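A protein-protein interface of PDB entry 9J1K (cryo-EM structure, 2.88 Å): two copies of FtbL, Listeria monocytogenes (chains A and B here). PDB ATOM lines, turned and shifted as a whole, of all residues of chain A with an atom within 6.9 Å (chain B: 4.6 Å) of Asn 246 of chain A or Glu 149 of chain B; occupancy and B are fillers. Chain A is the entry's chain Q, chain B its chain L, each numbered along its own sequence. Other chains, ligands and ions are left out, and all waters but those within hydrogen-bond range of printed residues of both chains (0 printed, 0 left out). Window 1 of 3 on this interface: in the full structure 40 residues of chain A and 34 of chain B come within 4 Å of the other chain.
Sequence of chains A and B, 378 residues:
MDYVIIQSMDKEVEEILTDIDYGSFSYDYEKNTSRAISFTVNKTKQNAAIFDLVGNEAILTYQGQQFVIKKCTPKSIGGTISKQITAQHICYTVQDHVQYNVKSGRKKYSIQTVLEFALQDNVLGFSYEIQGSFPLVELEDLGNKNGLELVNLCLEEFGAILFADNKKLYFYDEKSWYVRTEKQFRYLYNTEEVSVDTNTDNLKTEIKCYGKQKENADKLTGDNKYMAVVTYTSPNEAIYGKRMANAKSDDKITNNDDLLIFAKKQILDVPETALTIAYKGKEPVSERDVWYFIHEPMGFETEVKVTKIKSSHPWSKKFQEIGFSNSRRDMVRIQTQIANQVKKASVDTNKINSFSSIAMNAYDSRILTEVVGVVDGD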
ATOM      1  N   LYS A 204       3.090  36.635 -17.262  1.00  0.00           N
ATOM      2  CA  LYS A 204       4.465  36.169 -17.343  1.00  0.00           C
ATOM      3  C   LYS A 204       5.407  37.362 -17.306  1.00  0.00           C
ATOM      4  O   LYS A 204       5.160  38.378 -17.963  1.00  0.00           O
ATOM      5  CB  LYS A 204       4.699  35.350 -18.615  1.00  0.00           C
ATOM      6  CG  LYS A 204       3.763  34.165 -18.762  1.00  0.00           C
ATOM      7  CD  LYS A 204       3.921  33.193 -17.606  1.00  0.00           C
ATOM      8  CE  LYS A 204       3.297  31.846 -17.928  1.00  0.00           C
ATOM      9  NZ  LYS A 204       3.227  30.970 -16.727  1.00  0.00           N
ATOM     10  N   GLU A 206       9.018  36.794 -17.480  1.00  0.00           N
ATOM     11  CA  GLU A 206      10.329  36.352 -17.931  1.00  0.00           C
ATOM     12  C   GLU A 206      10.153  35.491 -19.171  1.00  0.00           C
ATOM     13  O   GLU A 206       9.166  34.762 -19.292  1.00  0.00           O
ATOM     14  CB  GLU A 206      11.061  35.573 -16.832  1.00  0.00           C
ATOM     15  CG  GLU A 206      12.446  35.090 -17.221  1.00  0.00           C
ATOM     16  CD  GLU A 206      13.402  35.057 -16.047  1.00  0.00           C
ATOM     17  OE1 GLU A 206      13.992  36.111 -15.731  1.00  0.00           O
ATOM     18  OE2 GLU A 206      13.561  33.979 -15.437  1.00  0.00           O
ATOM     19  N   ILE A 207      11.110  35.584 -20.093  1.00  0.00           N
ATOM     20  CA  ILE A 207      11.036  34.845 -21.345  1.00  0.00           C
ATOM     21  C   ILE A 207      12.448  34.599 -21.854  1.00  0.00           C
ATOM     22  O   ILE A 207      13.364  35.386 -21.602  1.00  0.00           O
ATOM     23  CB  ILE A 207      10.180  35.598 -22.390  1.00  0.00           C
ATOM     24  CG1 ILE A 207       9.877  34.706 -23.596  1.00  0.00           C
ATOM     25  CG2 ILE A 207      10.860  36.887 -22.816  1.00  0.00           C
ATOM     26  CD1 ILE A 207       9.255  33.386 -23.227  1.00  0.00           C
ATOM     27  N   LYS A 208      12.625  33.483 -22.555  1.00  0.00           N
ATOM     28  CA  LYS A 208      13.879  33.149 -23.218  1.00  0.00           C
ATOM     29  C   LYS A 208      13.607  32.961 -24.701  1.00  0.00           C
ATOM     30  O   LYS A 208      12.670  32.250 -25.077  1.00  0.00           O
ATOM     31  CB  LYS A 208      14.502  31.885 -22.623  1.00  0.00           C
ATOM     32  CG  LYS A 208      15.916  31.610 -23.100  1.00  0.00           C
ATOM     33  CD  LYS A 208      16.603  30.581 -22.220  1.00  0.00           C
ATOM     34  CE  LYS A 208      18.052  30.385 -22.628  1.00  0.00           C
ATOM     35  NZ  LYS A 208      18.745  29.403 -21.750  1.00  0.00           N
ATOM     36  N   CYS A 209      14.422  33.594 -25.540  1.00  0.00           N
ATOM     37  CA  CYS A 209      14.222  33.569 -26.979  1.00  0.00           C
ATOM     38  C   CYS A 209      15.533  33.255 -27.683  1.00  0.00           C
ATOM     39  O   CYS A 209      16.619  33.622 -27.216  1.00  0.00           O
ATOM     40  CB  CYS A 209      13.660  34.900 -27.491  1.00  0.00           C
ATOM     41  SG  CYS A 209      11.862  35.034 -27.380  1.00  0.00           S
ATOM     42  N   MET A 244       8.255  32.766 -15.661  1.00  0.00           N
ATOM     43  CA  MET A 244       8.804  32.565 -16.993  1.00  0.00           C
ATOM     44  C   MET A 244       7.892  31.667 -17.816  1.00  0.00           C
ATOM     45  O   MET A 244       7.294  30.721 -17.295  1.00  0.00           O
ATOM     46  CB  MET A 244      10.210  31.971 -16.912  1.00  0.00           C
ATOM     47  CG  MET A 244      10.378  30.874 -15.878  1.00  0.00           C
ATOM     48  SD  MET A 244      12.100  30.714 -15.373  1.00  0.00           S
ATOM     49  CE  MET A 244      12.095  29.090 -14.622  1.00  0.00           C
ATOM     50  N   ALA A 245       7.782  31.979 -19.102  1.00  0.00           N
ATOM     51  CA  ALA A 245       6.915  31.271 -20.029  1.00  0.00           C
ATOM     52  C   ALA A 245       7.742  30.373 -20.940  1.00  0.00           C
ATOM     53  O   ALA A 245       8.975  30.353 -20.888  1.00  0.00           O
ATOM     54  CB  ALA A 245       6.082  32.261 -20.846  1.00  0.00           C
ATOM     55  N   ASN A 246       7.043  29.617 -21.783  1.00  0.00           N
ATOM     56  CA  ASN A 246       7.708  28.727 -22.723  1.00  0.00           C
ATOM     57  C   ASN A 246       8.488  29.528 -23.756  1.00  0.00           C
ATOM     58  O   ASN A 246       8.047  30.588 -24.208  1.00  0.00           O
ATOM     59  CB  ASN A 246       6.687  27.827 -23.414  1.00  0.00           C
ATOM     60  CG  ASN A 246       6.176  26.727 -22.507  1.00  0.00           C
ATOM     61  OD1 ASN A 246       5.659  26.992 -21.422  1.00  0.00           O
ATOM     62  ND2 ASN A 246       6.318  25.483 -22.948  1.00  0.00           N
ATOM     63  N   ALA A 247       9.655  29.011 -24.130  1.00  0.00           N
ATOM     64  CA  ALA A 247      10.543  29.730 -25.032  1.00  0.00           C
ATOM     65  C   ALA A 247       9.927  29.865 -26.419  1.00  0.00           C
ATOM     66  O   ALA A 247       9.306  28.933 -26.937  1.00  0.00           O
ATOM     67  CB  ALA A 247      11.890  29.017 -25.127  1.00  0.00           C
ATOM     68  N   LYS A 248      10.103  31.039 -27.017  1.00  0.00           N
ATOM     69  CA  LYS A 248       9.674  31.315 -28.379  1.00  0.00           C
ATOM     70  C   LYS A 248      10.900  31.492 -29.264  1.00  0.00           C
ATOM     71  O   LYS A 248      11.880  32.127 -28.862  1.00  0.00           O
ATOM     72  CB  LYS A 248       8.798  32.568 -28.442  1.00  0.00           C
ATOM     73  CG  LYS A 248       7.500  32.462 -27.661  1.00  0.00           C
ATOM     74  CD  LYS A 248       6.370  31.946 -28.535  1.00  0.00           C
ATOM     75  CE  LYS A 248       5.366  31.146 -27.722  1.00  0.00           C
ATOM     76  NZ  LYS A 248       5.162  29.782 -28.283  1.00  0.00           N
ATOM     77  N   SER A 249      10.845  30.929 -30.468  1.00  0.00           N
ATOM     78  CA  SER A 249      11.979  30.920 -31.379  1.00  0.00           C
ATOM     79  C   SER A 249      11.631  31.672 -32.654  1.00  0.00           C
ATOM     80  O   SER A 249      10.611  31.385 -33.290  1.00  0.00           O
ATOM     81  CB  SER A 249      12.402  29.487 -31.714  1.00  0.00           C
ATOM     82  OG  SER A 249      12.674  28.748 -30.536  1.00  0.00           O
ATOM     83  N   ILE A 267       5.492  38.559 -24.537  1.00  0.00           N
ATOM     84  CA  ILE A 267       4.882  38.254 -23.250  1.00  0.00           C
ATOM     85  C   ILE A 267       3.970  39.398 -22.831  1.00  0.00           C
ATOM     86  O   ILE A 267       3.952  40.471 -23.434  1.00  0.00           O
ATOM     87  CB  ILE A 267       5.926  37.974 -22.148  1.00  0.00           C
ATOM     88  CG1 ILE A 267       6.747  39.228 -21.853  1.00  0.00           C
ATOM     89  CG2 ILE A 267       6.815  36.811 -22.541  1.00  0.00           C
ATOM     90  CD1 ILE A 267       7.502  39.162 -20.545  1.00  0.00           C
ATOM     91  N   VAL B  98       9.925  26.991 -15.857  1.00  0.00           N
ATOM     92  CA  VAL B  98      10.151  26.354 -17.148  1.00  0.00           C
ATOM     93  C   VAL B  98      11.571  25.812 -17.186  1.00  0.00           C
ATOM     94  O   VAL B  98      12.523  26.527 -16.855  1.00  0.00           O
ATOM     95  CB  VAL B  98       9.912  27.331 -18.314  1.00  0.00           C
ATOM     96  CG1 VAL B  98      10.143  26.635 -19.644  1.00  0.00           C
ATOM     97  CG2 VAL B  98       8.509  27.900 -18.246  1.00  0.00           C
ATOM     98  N   ASN B 144      12.355  21.500 -22.355  1.00  0.00           N
ATOM     99  CA  ASN B 144      11.765  22.622 -23.087  1.00  0.00           C
ATOM    100  C   ASN B 144      10.273  22.760 -22.791  1.00  0.00           C
ATOM    101  O   ASN B 144       9.469  23.065 -23.675  1.00  0.00           O
ATOM    102  CB  ASN B 144      12.012  22.493 -24.592  1.00  0.00           C
ATOM    103  CG  ASN B 144      11.896  23.817 -25.316  1.00  0.00           C
ATOM    104  OD1 ASN B 144      12.260  24.863 -24.781  1.00  0.00           O
ATOM    105  ND2 ASN B 144      11.386  23.778 -26.541  1.00  0.00           N
ATOM    106  N   LYS B 145       9.899  22.533 -21.535  1.00  0.00           N
ATOM    107  CA  LYS B 145       8.515  22.646 -21.099  1.00  0.00           C
ATOM    108  C   LYS B 145       8.482  23.224 -19.692  1.00  0.00           C
ATOM    109  O   LYS B 145       9.477  23.198 -18.965  1.00  0.00           O
ATOM    110  CB  LYS B 145       7.794  21.292 -21.122  1.00  0.00           C
ATOM    111  CG  LYS B 145       7.562  20.722 -22.511  1.00  0.00           C
ATOM    112  CD  LYS B 145       6.971  19.325 -22.431  1.00  0.00           C
ATOM    113  CE  LYS B 145       6.914  18.671 -23.799  1.00  0.00           C
ATOM    114  NZ  LYS B 145       6.049  17.460 -23.793  1.00  0.00           N
ATOM    115  N   ASN B 146       7.320  23.750 -19.316  1.00  0.00           N
ATOM    116  CA  ASN B 146       7.143  24.252 -17.965  1.00  0.00           C
ATOM    117  C   ASN B 146       6.948  23.091 -16.991  1.00  0.00           C
ATOM    118  O   ASN B 146       6.862  21.924 -17.380  1.00  0.00           O
ATOM    119  CB  ASN B 146       5.962  25.222 -17.899  1.00  0.00           C
ATOM    120  CG  ASN B 146       4.654  24.583 -18.321  1.00  0.00           C
ATOM    121  OD1 ASN B 146       4.139  23.687 -17.651  1.00  0.00           O
ATOM    122  ND2 ASN B 146       4.107  25.047 -19.436  1.00  0.00           N
ATOM    123  N   GLY B 147       6.884  23.429 -15.703  1.00  0.00           N
ATOM    124  CA  GLY B 147       6.750  22.399 -14.686  1.00  0.00           C
ATOM    125  C   GLY B 147       5.453  21.622 -14.799  1.00  0.00           C
ATOM    126  O   GLY B 147       5.442  20.394 -14.678  1.00  0.00           O
ATOM    127  N   LEU B 148       4.342  22.325 -15.033  1.00  0.00           N
ATOM    128  CA  LEU B 148       3.048  21.654 -15.099  1.00  0.00           C
ATOM    129  C   LEU B 148       2.968  20.711 -16.291  1.00  0.00           C
ATOM    130  O   LEU B 148       2.375  19.632 -16.193  1.00  0.00           O
ATOM    131  CB  LEU B 148       1.922  22.684 -15.156  1.00  0.00           C
ATOM    132  CG  LEU B 148       0.511  22.189 -14.836  1.00  0.00           C
ATOM    133  CD1 LEU B 148       0.541  21.064 -13.813  1.00  0.00           C
ATOM    134  CD2 LEU B 148      -0.354  23.335 -14.343  1.00  0.00           C
ATOM    135  N   GLU B 149       3.548  21.101 -17.428  1.00  0.00           N
ATOM    136  CA  GLU B 149       3.540  20.220 -18.591  1.00  0.00           C
ATOM    137  C   GLU B 149       4.296  18.929 -18.305  1.00  0.00           C
ATOM    138  O   GLU B 149       3.833  17.839 -18.656  1.00  0.00           O
ATOM    139  CB  GLU B 149       4.140  20.934 -19.802  1.00  0.00           C
ATOM    140  CG  GLU B 149       3.141  21.763 -20.589  1.00  0.00           C
ATOM    141  CD  GLU B 149       3.810  22.722 -21.552  1.00  0.00           C
ATOM    142  OE1 GLU B 149       4.754  23.425 -21.135  1.00  0.00           O
ATOM    143  OE2 GLU B 149       3.393  22.774 -22.728  1.00  0.00           O
ATOM    144  N   LEU B 150       5.455  19.031 -17.652  1.00  0.00           N
ATOM    145  CA  LEU B 150       6.223  17.835 -17.327  1.00  0.00           C
ATOM    146  C   LEU B 150       5.511  16.984 -16.283  1.00  0.00           C
ATOM    147  O   LEU B 150       5.559  15.751 -16.343  1.00  0.00           O
ATOM    148  CB  LEU B 150       7.620  18.227 -16.852  1.00  0.00           C
ATOM    149  CG  LEU B 150       8.516  18.799 -17.952  1.00  0.00           C
ATOM    150  CD1 LEU B 150       9.634  19.644 -17.368  1.00  0.00           C
ATOM    151  CD2 LEU B 150       9.078  17.681 -18.814  1.00  0.00           C
ATOM    152  N   VAL B 151       4.840  17.621 -15.321  1.00  0.00           N
ATOM    153  CA  VAL B 151       4.080  16.866 -14.327  1.00  0.00           C
ATOM    154  C   VAL B 151       2.937  16.107 -14.993  1.00  0.00           C
ATOM    155  O   VAL B 151       2.685  14.935 -14.686  1.00  0.00           O
ATOM    156  CB  VAL B 151       3.570  17.805 -13.219  1.00  0.00           C
ATOM    157  CG1 VAL B 151       2.525  17.108 -12.367  1.00  0.00           C
ATOM    158  CG2 VAL B 151       4.728  18.276 -12.356  1.00  0.00           C
ATOM    159  N   ASN B 152       2.230  16.763 -15.917  1.00  0.00           N
ATOM    160  CA  ASN B 152       1.160  16.091 -16.645  1.00  0.00           C
ATOM    161  C   ASN B 152       1.706  14.959 -17.502  1.00  0.00           C
ATOM    162  O   ASN B 152       1.074  13.904 -17.628  1.00  0.00           O
ATOM    163  CB  ASN B 152       0.398  17.099 -17.504  1.00  0.00           C
ATOM    164  CG  ASN B 152      -0.518  17.985 -16.687  1.00  0.00           C
ATOM    165  OD1 ASN B 152      -0.829  17.681 -15.536  1.00  0.00           O
ATOM    166  ND2 ASN B 152      -0.955  19.089 -17.279  1.00  0.00           N
ATOM    167  N   LEU B 153       2.879  15.162 -18.106  1.00  0.00           N
ATOM    168  CA  LEU B 153       3.513  14.093 -18.868  1.00  0.00           C
ATOM    169  C   LEU B 153       3.829  12.898 -17.980  1.00  0.00           C
ATOM    170  O   LEU B 153       3.601  11.747 -18.369  1.00  0.00           O
ATOM    171  CB  LEU B 153       4.784  14.613 -19.538  1.00  0.00           C
ATOM    172  CG  LEU B 153       5.595  13.599 -20.344  1.00  0.00           C
ATOM    173  CD1 LEU B 153       4.879  13.248 -21.635  1.00  0.00           C
ATOM    174  CD2 LEU B 153       6.988  14.134 -20.626  1.00  0.00           C
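No position is printed for both chains.
Of the 4 pairs that touch across the chains among the printed residues, none has its exchanged pair printed and touching as well.
Of the 11 printed residues of chain B, 3 touch a printed residue of chain A.
Hydrophobic or aromatic side chains of chain A within 4 Å of the printed part of chain B: Met 244.
Along chain A the printed residues that touch a printed residue of chain B span positions 244 to 246.
Among the printed residues, 4 pairs touch across the chains.
OE1 of Glu 149 of chain B is in hydrogen-bond range of ND2 of Asn 246 of chain A (3.2 Å).
OD1 of Asn 246 of chain A lies within hydrogen-bond range of ND2 of Asn 146 of chain B, 3.2 Å away.
The side-chain amide oxygen (OD1) of Asn 146 of chain B sits at hydrogen-bond distance from the backbone NH (N) of Leu 148 of chain B (3.0 Å).
The backbone carbonyl oxygen (O) of Glu 206 of chain A sits at hydrogen-bond distance from the backbone NH (N) of Ala 245 of chain A (3.1 Å).
OE1 of Glu 149 of chain B is in hydrogen-bond range of ND2 of Asn 146 of chain B (2.4 Å).
Printed residues of chain B within 4 Å of Met 244 of chain A: Val 98.
Printed residues of chain B within 4 Å of Ala 245 of chain A: Val 98.
Of chain B, only Asn 146 (3.2 Å) and Glu 149 (3.2 Å) come within 4 Å of Asn 246 of chain A.
Printed residues of chain A within 4 Å of Val 98 of chain B: Met 244 (3.2 Å) and Ala 245 (3.6 Å).
Of the printed residues of chain A, Asn 146 of chain B touches Asn 246 (3.2 Å).
Of chain A, only Asn 246 comes within 4 Å of Glu 149 of chain B.
Among the printed residues, pairs that only touch across the chains: Met 244 of chain A with Val 98 of chain B (3.2 Å) and Ala 245 of chain A with Val 98 of chain B (3.6 Å).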
